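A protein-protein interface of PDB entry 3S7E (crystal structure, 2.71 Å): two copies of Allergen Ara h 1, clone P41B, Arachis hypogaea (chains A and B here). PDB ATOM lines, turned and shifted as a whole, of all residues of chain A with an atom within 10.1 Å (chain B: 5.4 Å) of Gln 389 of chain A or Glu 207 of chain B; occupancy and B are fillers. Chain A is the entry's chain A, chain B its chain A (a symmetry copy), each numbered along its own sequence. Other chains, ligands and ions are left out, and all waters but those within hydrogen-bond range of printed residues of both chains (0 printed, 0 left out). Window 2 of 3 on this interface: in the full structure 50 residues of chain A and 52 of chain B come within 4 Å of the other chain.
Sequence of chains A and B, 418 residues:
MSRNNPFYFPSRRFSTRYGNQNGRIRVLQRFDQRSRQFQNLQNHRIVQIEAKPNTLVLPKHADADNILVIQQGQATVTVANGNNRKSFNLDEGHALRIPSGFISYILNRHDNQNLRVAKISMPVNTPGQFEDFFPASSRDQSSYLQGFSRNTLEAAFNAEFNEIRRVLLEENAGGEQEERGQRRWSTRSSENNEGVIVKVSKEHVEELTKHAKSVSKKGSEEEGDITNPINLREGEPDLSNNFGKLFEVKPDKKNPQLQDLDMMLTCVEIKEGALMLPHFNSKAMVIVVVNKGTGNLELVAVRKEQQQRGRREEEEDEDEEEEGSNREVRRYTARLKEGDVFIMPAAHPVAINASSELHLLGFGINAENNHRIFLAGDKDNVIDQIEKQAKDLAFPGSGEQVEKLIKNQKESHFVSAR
The side-chain amide oxygen of Gln 389 of chain A lies close to the backbone carbonyl oxygen of His 204 of chain B, 3.4 Å away.
The side-chain carboxylate of Glu 207 of chain B sits at hydrogen-bond distance from the side-chain amide nitrogen of Gln 389 of chain A (2.8 Å).
The side-chain amide oxygen (OE1) of Gln 389 of chain A lies within hydrogen-bond range of the backbone NH (N) of Leu 208 of chain B, 3.0 Å away.
The side-chain carboxylate (OE1) of Glu 387 of chain A sits close to the backbone carbonyl oxygen (O) of His 211 of chain B, at 3.4 Å.
Of the 9 printed residues of chain B, 4 touch a printed residue of chain A.
Hydrophobic or aromatic side chains of chain B that line the printed part of chain A: Leu 208.
Among the printed residues, no Asp or Glu carboxylate lies within 4 Å of a Lys or Arg side-chain nitrogen of the other chain.
Glu 387 of chain A touches Leu 208 of chain B (OE2 to CD2, 3.2 Å).
No position is printed for both chains.
Of the 5 pairs that touch across the chains among the printed residues, none has its exchanged pair printed and touching as well.
Gln 389 of chain A touches three residues of chain B.
Glu 207 of chain B touches just one residue of chain A: Gln 389 (2.8 Å).
His 204 of chain B touches one residue of chain A.
Leu 208 of chain B touches just these residues of chain A: Glu 387 (3.2 Å) and Gln 389 (3.0 Å).
No residue of chain A comes within 4 Å of Lys 210 of chain B.
Of the printed residues of chain A, His 211 of chain B touches Glu 387 (3.4 Å).
Of the printed residues of chain B, Glu 387 of chain A touches Leu 208 (3.2 Å) and His 211 (3.4 Å).
The nearest printed residue of chain B that does not touch Gln 389 of chain A is Val 205 of chain B (5.6 Å).
The nearest residue of chain A that does not touch Glu 207 of chain B is Glu 387 of chain A (4.9 Å).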
ATOM      1  N   ILE A 383      -5.571 -19.808  18.144  1.00  0.00           N
ATOM      2  CA  ILE A 383      -4.119 -20.040  18.049  1.00  0.00           C
ATOM      3  C   ILE A 383      -3.654 -21.110  19.025  1.00  0.00           C
ATOM      4  O   ILE A 383      -2.907 -22.004  18.655  1.00  0.00           O
ATOM      5  CB  ILE A 383      -3.295 -18.769  18.328  1.00  0.00           C
ATOM      6  CG1 ILE A 383      -3.574 -17.715  17.253  1.00  0.00           C
ATOM      7  CG2 ILE A 383      -1.802 -19.096  18.360  1.00  0.00           C
ATOM      8  CD1 ILE A 383      -2.720 -16.472  17.388  1.00  0.00           C
ATOM      9  N   ASP A 384      -4.109 -21.006  20.270  1.00  0.00           N
ATOM     10  CA  ASP A 384      -3.905 -22.053  21.284  1.00  0.00           C
ATOM     11  C   ASP A 384      -4.133 -23.476  20.723  1.00  0.00           C
ATOM     12  O   ASP A 384      -3.357 -24.388  21.016  1.00  0.00           O
ATOM     13  CB  ASP A 384      -4.837 -21.791  22.476  1.00  0.00           C
ATOM     14  CG  ASP A 384      -4.861 -22.940  23.482  1.00  0.00           C
ATOM     15  OD1 ASP A 384      -3.787 -23.493  23.806  1.00  0.00           O
ATOM     16  OD2 ASP A 384      -5.967 -23.281  23.959  1.00  0.00           O
ATOM     17  N   GLN A 385      -5.185 -23.643  19.915  1.00  0.00           N
ATOM     18  CA  GLN A 385      -5.580 -24.962  19.364  1.00  0.00           C
ATOM     19  C   GLN A 385      -4.616 -25.552  18.336  1.00  0.00           C
ATOM     20  O   GLN A 385      -4.560 -26.763  18.180  1.00  0.00           O
ATOM     21  CB  GLN A 385      -6.981 -24.906  18.747  1.00  0.00           C
ATOM     22  CG  GLN A 385      -8.072 -24.556  19.732  1.00  0.00           C
ATOM     23  CD  GLN A 385      -8.247 -25.619  20.802  1.00  0.00           C
ATOM     24  OE1 GLN A 385      -8.707 -26.729  20.522  1.00  0.00           O
ATOM     25  NE2 GLN A 385      -7.875 -25.286  22.038  1.00  0.00           N
ATOM     26  N   ILE A 386      -3.881 -24.703  17.625  1.00  0.00           N
ATOM     27  CA  ILE A 386      -2.833 -25.172  16.716  1.00  0.00           C
ATOM     28  C   ILE A 386      -1.909 -26.185  17.421  1.00  0.00           C
ATOM     29  O   ILE A 386      -1.539 -25.985  18.574  1.00  0.00           O
ATOM     30  CB  ILE A 386      -1.978 -23.988  16.188  1.00  0.00           C
ATOM     31  CG1 ILE A 386      -2.808 -23.076  15.281  1.00  0.00           C
ATOM     32  CG2 ILE A 386      -0.737 -24.492  15.441  1.00  0.00           C
ATOM     33  CD1 ILE A 386      -1.972 -22.164  14.396  1.00  0.00           C
ATOM     34  N   GLU A 387      -1.549 -27.272  16.735  1.00  0.00           N
ATOM     35  CA  GLU A 387      -0.562 -28.249  17.265  1.00  0.00           C
ATOM     36  C   GLU A 387       0.742 -27.561  17.661  1.00  0.00           C
ATOM     37  O   GLU A 387       1.153 -26.604  17.008  1.00  0.00           O
ATOM     38  CB  GLU A 387      -0.251 -29.361  16.247  1.00  0.00           C
ATOM     39  CG  GLU A 387      -1.359 -30.405  16.105  1.00  0.00           C
ATOM     40  CD  GLU A 387      -1.048 -31.476  15.079  1.00  0.00           C
ATOM     41  OE1 GLU A 387      -1.439 -32.643  15.315  1.00  0.00           O
ATOM     42  OE2 GLU A 387      -0.416 -31.158  14.043  1.00  0.00           O
ATOM     43  N   LYS A 388       1.388 -28.058  18.715  1.00  0.00           N
ATOM     44  CA  LYS A 388       2.625 -27.440  19.251  1.00  0.00           C
ATOM     45  C   LYS A 388       3.793 -27.374  18.244  1.00  0.00           C
ATOM     46  O   LYS A 388       4.485 -26.354  18.168  1.00  0.00           O
ATOM     47  CB  LYS A 388       3.069 -28.132  20.542  1.00  0.00           C
ATOM     48  CG  LYS A 388       4.254 -27.457  21.257  1.00  0.00           C
ATOM     49  CD  LYS A 388       4.396 -27.930  22.714  1.00  0.00           C
ATOM     50  CE  LYS A 388       5.842 -27.845  23.232  1.00  0.00           C
ATOM     51  NZ  LYS A 388       6.013 -28.557  24.530  1.00  0.00           N
ATOM     52  N   GLN A 389       4.005 -28.441  17.472  1.00  0.00           N
ATOM     53  CA  GLN A 389       5.008 -28.417  16.387  1.00  0.00           C
ATOM     54  C   GLN A 389       4.550 -27.525  15.249  1.00  0.00           C
ATOM     55  O   GLN A 389       5.366 -27.056  14.455  1.00  0.00           O
ATOM     56  CB  GLN A 389       5.260 -29.793  15.772  1.00  0.00           C
ATOM     57  CG  GLN A 389       6.093 -30.740  16.583  1.00  0.00           C
ATOM     58  CD  GLN A 389       5.286 -31.923  17.071  1.00  0.00           C
ATOM     59  OE1 GLN A 389       4.513 -32.520  16.311  1.00  0.00           O
ATOM     60  NE2 GLN A 389       5.467 -32.283  18.344  1.00  0.00           N
ATOM     61  N   ALA A 390       3.242 -27.339  15.136  1.00  0.00           N
ATOM     62  CA  ALA A 390       2.698 -26.469  14.103  1.00  0.00           C
ATOM     63  C   ALA A 390       3.120 -25.014  14.352  1.00  0.00           C
ATOM     64  O   ALA A 390       3.528 -24.322  13.422  1.00  0.00           O
ATOM     65  CB  ALA A 390       1.188 -26.596  14.029  1.00  0.00           C
ATOM     66  N   LYS A 391       3.043 -24.564  15.604  1.00  0.00           N
ATOM     67  CA  LYS A 391       3.425 -23.184  15.963  1.00  0.00           C
ATOM     68  C   LYS A 391       4.941 -22.926  15.848  1.00  0.00           C
ATOM     69  O   LYS A 391       5.375 -21.876  15.354  1.00  0.00           O
ATOM     70  CB  LYS A 391       2.926 -22.839  17.373  1.00  0.00           C
ATOM     71  CG  LYS A 391       1.403 -22.742  17.455  1.00  0.00           C
ATOM     72  CD  LYS A 391       0.884 -22.190  18.792  1.00  0.00           C
ATOM     73  CE  LYS A 391       0.489 -23.303  19.773  1.00  0.00           C
ATOM     74  NZ  LYS A 391      -0.473 -22.813  20.802  1.00  0.00           N
ATOM     75  N   ASP A 392       5.718 -23.909  16.299  1.00  0.00           N
ATOM     76  CA  ASP A 392       7.187 -23.869  16.296  1.00  0.00           C
ATOM     77  C   ASP A 392       7.773 -23.564  14.914  1.00  0.00           C
ATOM     78  O   ASP A 392       8.704 -22.765  14.787  1.00  0.00           O
ATOM     79  CB  ASP A 392       7.732 -25.211  16.806  1.00  0.00           C
ATOM     80  CG  ASP A 392       9.253 -25.277  16.802  1.00  0.00           C
ATOM     81  OD1 ASP A 392       9.881 -24.665  17.681  1.00  0.00           O
ATOM     82  OD2 ASP A 392       9.824 -25.967  15.934  1.00  0.00           O
ATOM     83  N   LEU A 393       7.227 -24.208  13.887  1.00  0.00           N
ATOM     84  CA  LEU A 393       7.712 -24.042  12.507  1.00  0.00           C
ATOM     85  C   LEU A 393       7.197 -22.759  11.857  1.00  0.00           C
ATOM     86  O   LEU A 393       7.960 -22.027  11.217  1.00  0.00           O
ATOM     87  CB  LEU A 393       7.309 -25.242  11.643  1.00  0.00           C
ATOM     88  CG  LEU A 393       8.051 -26.540  11.972  1.00  0.00           C
ATOM     89  CD1 LEU A 393       7.319 -27.728  11.388  1.00  0.00           C
ATOM     90  CD2 LEU A 393       9.502 -26.489  11.485  1.00  0.00           C
ATOM     91  N   ALA A 394       5.899 -22.517  12.009  1.00  0.00           N
ATOM     92  CA  ALA A 394       5.263 -21.313  11.479  1.00  0.00           C
ATOM     93  C   ALA A 394       5.869 -20.048  12.091  1.00  0.00           C
ATOM     94  O   ALA A 394       6.447 -19.224  11.378  1.00  0.00           O
ATOM     95  CB  ALA A 394       3.763 -21.353  11.726  1.00  0.00           C
ATOM     96  N   PHE A 395       5.759 -19.911  13.412  1.00  0.00           N
ATOM     97  CA  PHE A 395       6.180 -18.673  14.086  1.00  0.00           C
ATOM     98  C   PHE A 395       7.709 -18.544  14.260  1.00  0.00           C
ATOM     99  O   PHE A 395       8.419 -19.551  14.323  1.00  0.00           O
ATOM    100  CB  PHE A 395       5.475 -18.530  15.438  1.00  0.00           C
ATOM    101  CG  PHE A 395       3.980 -18.581  15.342  1.00  0.00           C
ATOM    102  CD1 PHE A 395       3.258 -19.460  16.121  1.00  0.00           C
ATOM    103  CD2 PHE A 395       3.300 -17.767  14.456  1.00  0.00           C
ATOM    104  CE1 PHE A 395       1.889 -19.516  16.035  1.00  0.00           C
ATOM    105  CE2 PHE A 395       1.926 -17.824  14.362  1.00  0.00           C
ATOM    106  CZ  PHE A 395       1.222 -18.702  15.151  1.00  0.00           C
ATOM    107  N   GLY A 397       9.516 -17.671  16.875  1.00  0.00           N
ATOM    108  CA  GLY A 397       9.930 -18.328  18.106  1.00  0.00           C
ATOM    109  C   GLY A 397       9.811 -19.843  18.107  1.00  0.00           C
ATOM    110  O   GLY A 397       9.272 -20.460  17.180  1.00  0.00           O
ATOM    111  N   SER A 398      10.344 -20.437  19.168  1.00  0.00           N
ATOM    112  CA  SER A 398      10.137 -21.846  19.452  1.00  0.00           C
ATOM    113  C   SER A 398       8.685 -22.071  19.765  1.00  0.00           C
ATOM    114  O   SER A 398       7.915 -21.122  19.862  1.00  0.00           O
ATOM    115  CB  SER A 398      10.958 -22.296  20.653  1.00  0.00           C
ATOM    116  OG  SER A 398      10.800 -21.398  21.738  1.00  0.00           O
ATOM    117  N   GLY A 399       8.318 -23.333  19.937  1.00  0.00           N
ATOM    118  CA  GLY A 399       6.938 -23.700  20.225  1.00  0.00           C
ATOM    119  C   GLY A 399       6.545 -23.384  21.652  1.00  0.00           C
ATOM    120  O   GLY A 399       5.529 -22.736  21.891  1.00  0.00           O
ATOM    121  N   GLU A 400       7.376 -23.820  22.591  1.00  0.00           N
ATOM    122  CA  GLU A 400       7.094 -23.662  24.032  1.00  0.00           C
ATOM    123  C   GLU A 400       7.035 -22.194  24.468  1.00  0.00           C
ATOM    124  O   GLU A 400       6.269 -21.837  25.362  1.00  0.00           O
ATOM    125  CB  GLU A 400       8.154 -24.401  24.859  1.00  0.00           C
ATOM    126  N   VAL A 402       6.392 -19.458  22.215  1.00  0.00           N
ATOM    127  CA  VAL A 402       5.144 -19.018  21.565  1.00  0.00           C
ATOM    128  C   VAL A 402       3.887 -19.498  22.291  1.00  0.00           C
ATOM    129  O   VAL A 402       2.882 -18.785  22.358  1.00  0.00           O
ATOM    130  CB  VAL A 402       5.078 -19.543  20.103  1.00  0.00           C
ATOM    131  CG1 VAL A 402       3.650 -19.738  19.658  1.00  0.00           C
ATOM    132  CG2 VAL A 402       5.800 -18.597  19.157  1.00  0.00           C
ATOM    133  N   GLU A 403       3.946 -20.713  22.810  1.00  0.00           N
ATOM    134  CA  GLU A 403       2.851 -21.265  23.601  1.00  0.00           C
ATOM    135  C   GLU A 403       2.772 -20.629  24.996  1.00  0.00           C
ATOM    136  O   GLU A 403       1.704 -20.618  25.619  1.00  0.00           O
ATOM    137  CB  GLU A 403       3.006 -22.777  23.712  1.00  0.00           C
ATOM    138  CG  GLU A 403       1.771 -23.516  24.184  1.00  0.00           C
ATOM    139  CD  GLU A 403       1.804 -24.973  23.783  1.00  0.00           C
ATOM    140  OE1 GLU A 403       2.267 -25.265  22.661  1.00  0.00           O
ATOM    141  OE2 GLU A 403       1.379 -25.828  24.589  1.00  0.00           O
ATOM    142  N   GLU B 203      11.638 -36.583  13.020  1.00  0.00           N
ATOM    143  CA  GLU B 203      11.156 -36.702  14.392  1.00  0.00           C
ATOM    144  C   GLU B 203       9.926 -35.820  14.630  1.00  0.00           C
ATOM    145  O   GLU B 203       8.930 -36.280  15.190  1.00  0.00           O
ATOM    146  CB  GLU B 203      12.282 -36.311  15.356  1.00  0.00           C
ATOM    147  CG  GLU B 203      11.958 -36.449  16.835  1.00  0.00           C
ATOM    148  CD  GLU B 203      12.896 -35.628  17.697  1.00  0.00           C
ATOM    149  OE1 GLU B 203      13.502 -34.675  17.169  1.00  0.00           O
ATOM    150  OE2 GLU B 203      13.023 -35.927  18.900  1.00  0.00           O
ATOM    151  N   HIS B 204      10.012 -34.557  14.210  1.00  0.00           N
ATOM    152  CA  HIS B 204       8.866 -33.629  14.283  1.00  0.00           C
ATOM    153  C   HIS B 204       7.618 -34.289  13.673  1.00  0.00           C
ATOM    154  O   HIS B 204       6.537 -34.242  14.252  1.00  0.00           O
ATOM    155  CB  HIS B 204       9.165 -32.292  13.572  1.00  0.00           C
ATOM    156  CG  HIS B 204      10.128 -31.401  14.308  1.00  0.00           C
ATOM    157  ND1 HIS B 204      10.938 -30.494  13.661  1.00  0.00           N
ATOM    158  CD2 HIS B 204      10.412 -31.279  15.628  1.00  0.00           C
ATOM    159  CE1 HIS B 204      11.675 -29.847  14.550  1.00  0.00           C
ATOM    160  NE2 HIS B 204      11.378 -30.306  15.750  1.00  0.00           N
ATOM    161  N   VAL B 205       7.794 -34.914  12.509  1.00  0.00           N
ATOM    162  CA  VAL B 205       6.714 -35.634  11.803  1.00  0.00           C
ATOM    163  C   VAL B 205       6.050 -36.729  12.670  1.00  0.00           C
ATOM    164  O   VAL B 205       4.817 -36.879  12.671  1.00  0.00           O
ATOM    165  CB  VAL B 205       7.226 -36.255  10.455  1.00  0.00           C
ATOM    166  CG1 VAL B 205       6.260 -37.311   9.918  1.00  0.00           C
ATOM    167  CG2 VAL B 205       7.454 -35.170   9.417  1.00  0.00           C
ATOM    168  N   GLU B 206       6.858 -37.475  13.416  1.00  0.00           N
ATOM    169  CA  GLU B 206       6.338 -38.579  14.238  1.00  0.00           C
ATOM    170  C   GLU B 206       5.355 -38.115  15.331  1.00  0.00           C
ATOM    171  O   GLU B 206       4.553 -38.902  15.820  1.00  0.00           O
ATOM    172  CB  GLU B 206       7.483 -39.387  14.859  1.00  0.00           C
ATOM    173  CG  GLU B 206       8.357 -40.115  13.830  1.00  0.00           C
ATOM    174  CD  GLU B 206       9.543 -40.851  14.456  1.00  0.00           C
ATOM    175  OE1 GLU B 206       9.529 -41.084  15.687  1.00  0.00           O
ATOM    176  OE2 GLU B 206      10.485 -41.205  13.709  1.00  0.00           O
ATOM    177  N   GLU B 207       5.423 -36.844  15.707  1.00  0.00           N
ATOM    178  CA  GLU B 207       4.506 -36.278  16.704  1.00  0.00           C
ATOM    179  C   GLU B 207       3.249 -35.663  16.073  1.00  0.00           C
ATOM    180  O   GLU B 207       2.150 -35.794  16.613  1.00  0.00           O
ATOM    181  CB  GLU B 207       5.233 -35.236  17.538  1.00  0.00           C
ATOM    182  CG  GLU B 207       6.322 -35.817  18.430  1.00  0.00           C
ATOM    183  CD  GLU B 207       7.499 -34.887  18.601  1.00  0.00           C
ATOM    184  OE1 GLU B 207       8.268 -35.076  19.562  1.00  0.00           O
ATOM    185  OE2 GLU B 207       7.667 -33.968  17.772  1.00  0.00           O
ATOM    186  N   LEU B 208       3.425 -34.984  14.940  1.00  0.00           N
ATOM    187  CA  LEU B 208       2.304 -34.485  14.134  1.00  0.00           C
ATOM    188  C   LEU B 208       1.419 -35.641  13.695  1.00  0.00           C
ATOM    189  O   LEU B 208       0.188 -35.535  13.743  1.00  0.00           O
ATOM    190  CB  LEU B 208       2.801 -33.730  12.896  1.00  0.00           C
ATOM    191  CG  LEU B 208       3.612 -32.452  13.147  1.00  0.00           C
ATOM    192  CD1 LEU B 208       4.255 -31.949  11.862  1.00  0.00           C
ATOM    193  CD2 LEU B 208       2.737 -31.367  13.767  1.00  0.00           C
ATOM    194  N   THR B 209       2.056 -36.733  13.257  1.00  0.00           N
ATOM    195  CA  THR B 209       1.357 -38.001  12.952  1.00  0.00           C
ATOM    196  C   THR B 209       0.863 -38.713  14.202  1.00  0.00           C
ATOM    197  O   THR B 209      -0.207 -39.333  14.193  1.00  0.00           O
ATOM    198  CB  THR B 209       2.275 -39.011  12.248  1.00  0.00           C
ATOM    199  OG1 THR B 209       2.557 -38.558  10.922  1.00  0.00           O
ATOM    200  CG2 THR B 209       1.614 -40.390  12.175  1.00  0.00           C
ATOM    201  N   LYS B 210       1.678 -38.636  15.257  1.00  0.00           N
ATOM    202  CA  LYS B 210       1.364 -39.227  16.559  1.00  0.00           C
ATOM    203  C   LYS B 210      -0.082 -38.938  16.894  1.00  0.00           C
ATOM    204  O   LYS B 210      -0.878 -39.852  17.136  1.00  0.00           O
ATOM    205  CB  LYS B 210       2.254 -38.632  17.652  1.00  0.00           C
ATOM    206  N   HIS B 211      -0.409 -37.651  16.876  1.00  0.00           N
ATOM    207  CA  HIS B 211      -1.775 -37.189  17.066  1.00  0.00           C
ATOM    208  C   HIS B 211      -2.381 -37.014  15.665  1.00  0.00           C
ATOM    209  O   HIS B 211      -2.557 -35.894  15.175  1.00  0.00           O
ATOM    210  CB  HIS B 211      -1.789 -35.912  17.910  1.00  0.00           C
ATOM    211  CG  HIS B 211      -1.112 -36.077  19.235  1.00  0.00           C
ATOM    212  ND1 HIS B 211      -0.330 -35.093  19.803  1.00  0.00           N
ATOM    213  CD2 HIS B 211      -1.074 -37.128  20.088  1.00  0.00           C
ATOM    214  CE1 HIS B 211       0.149 -35.527  20.955  1.00  0.00           C
ATOM    215  NE2 HIS B 211      -0.287 -36.759  21.152  1.00  0.00           N
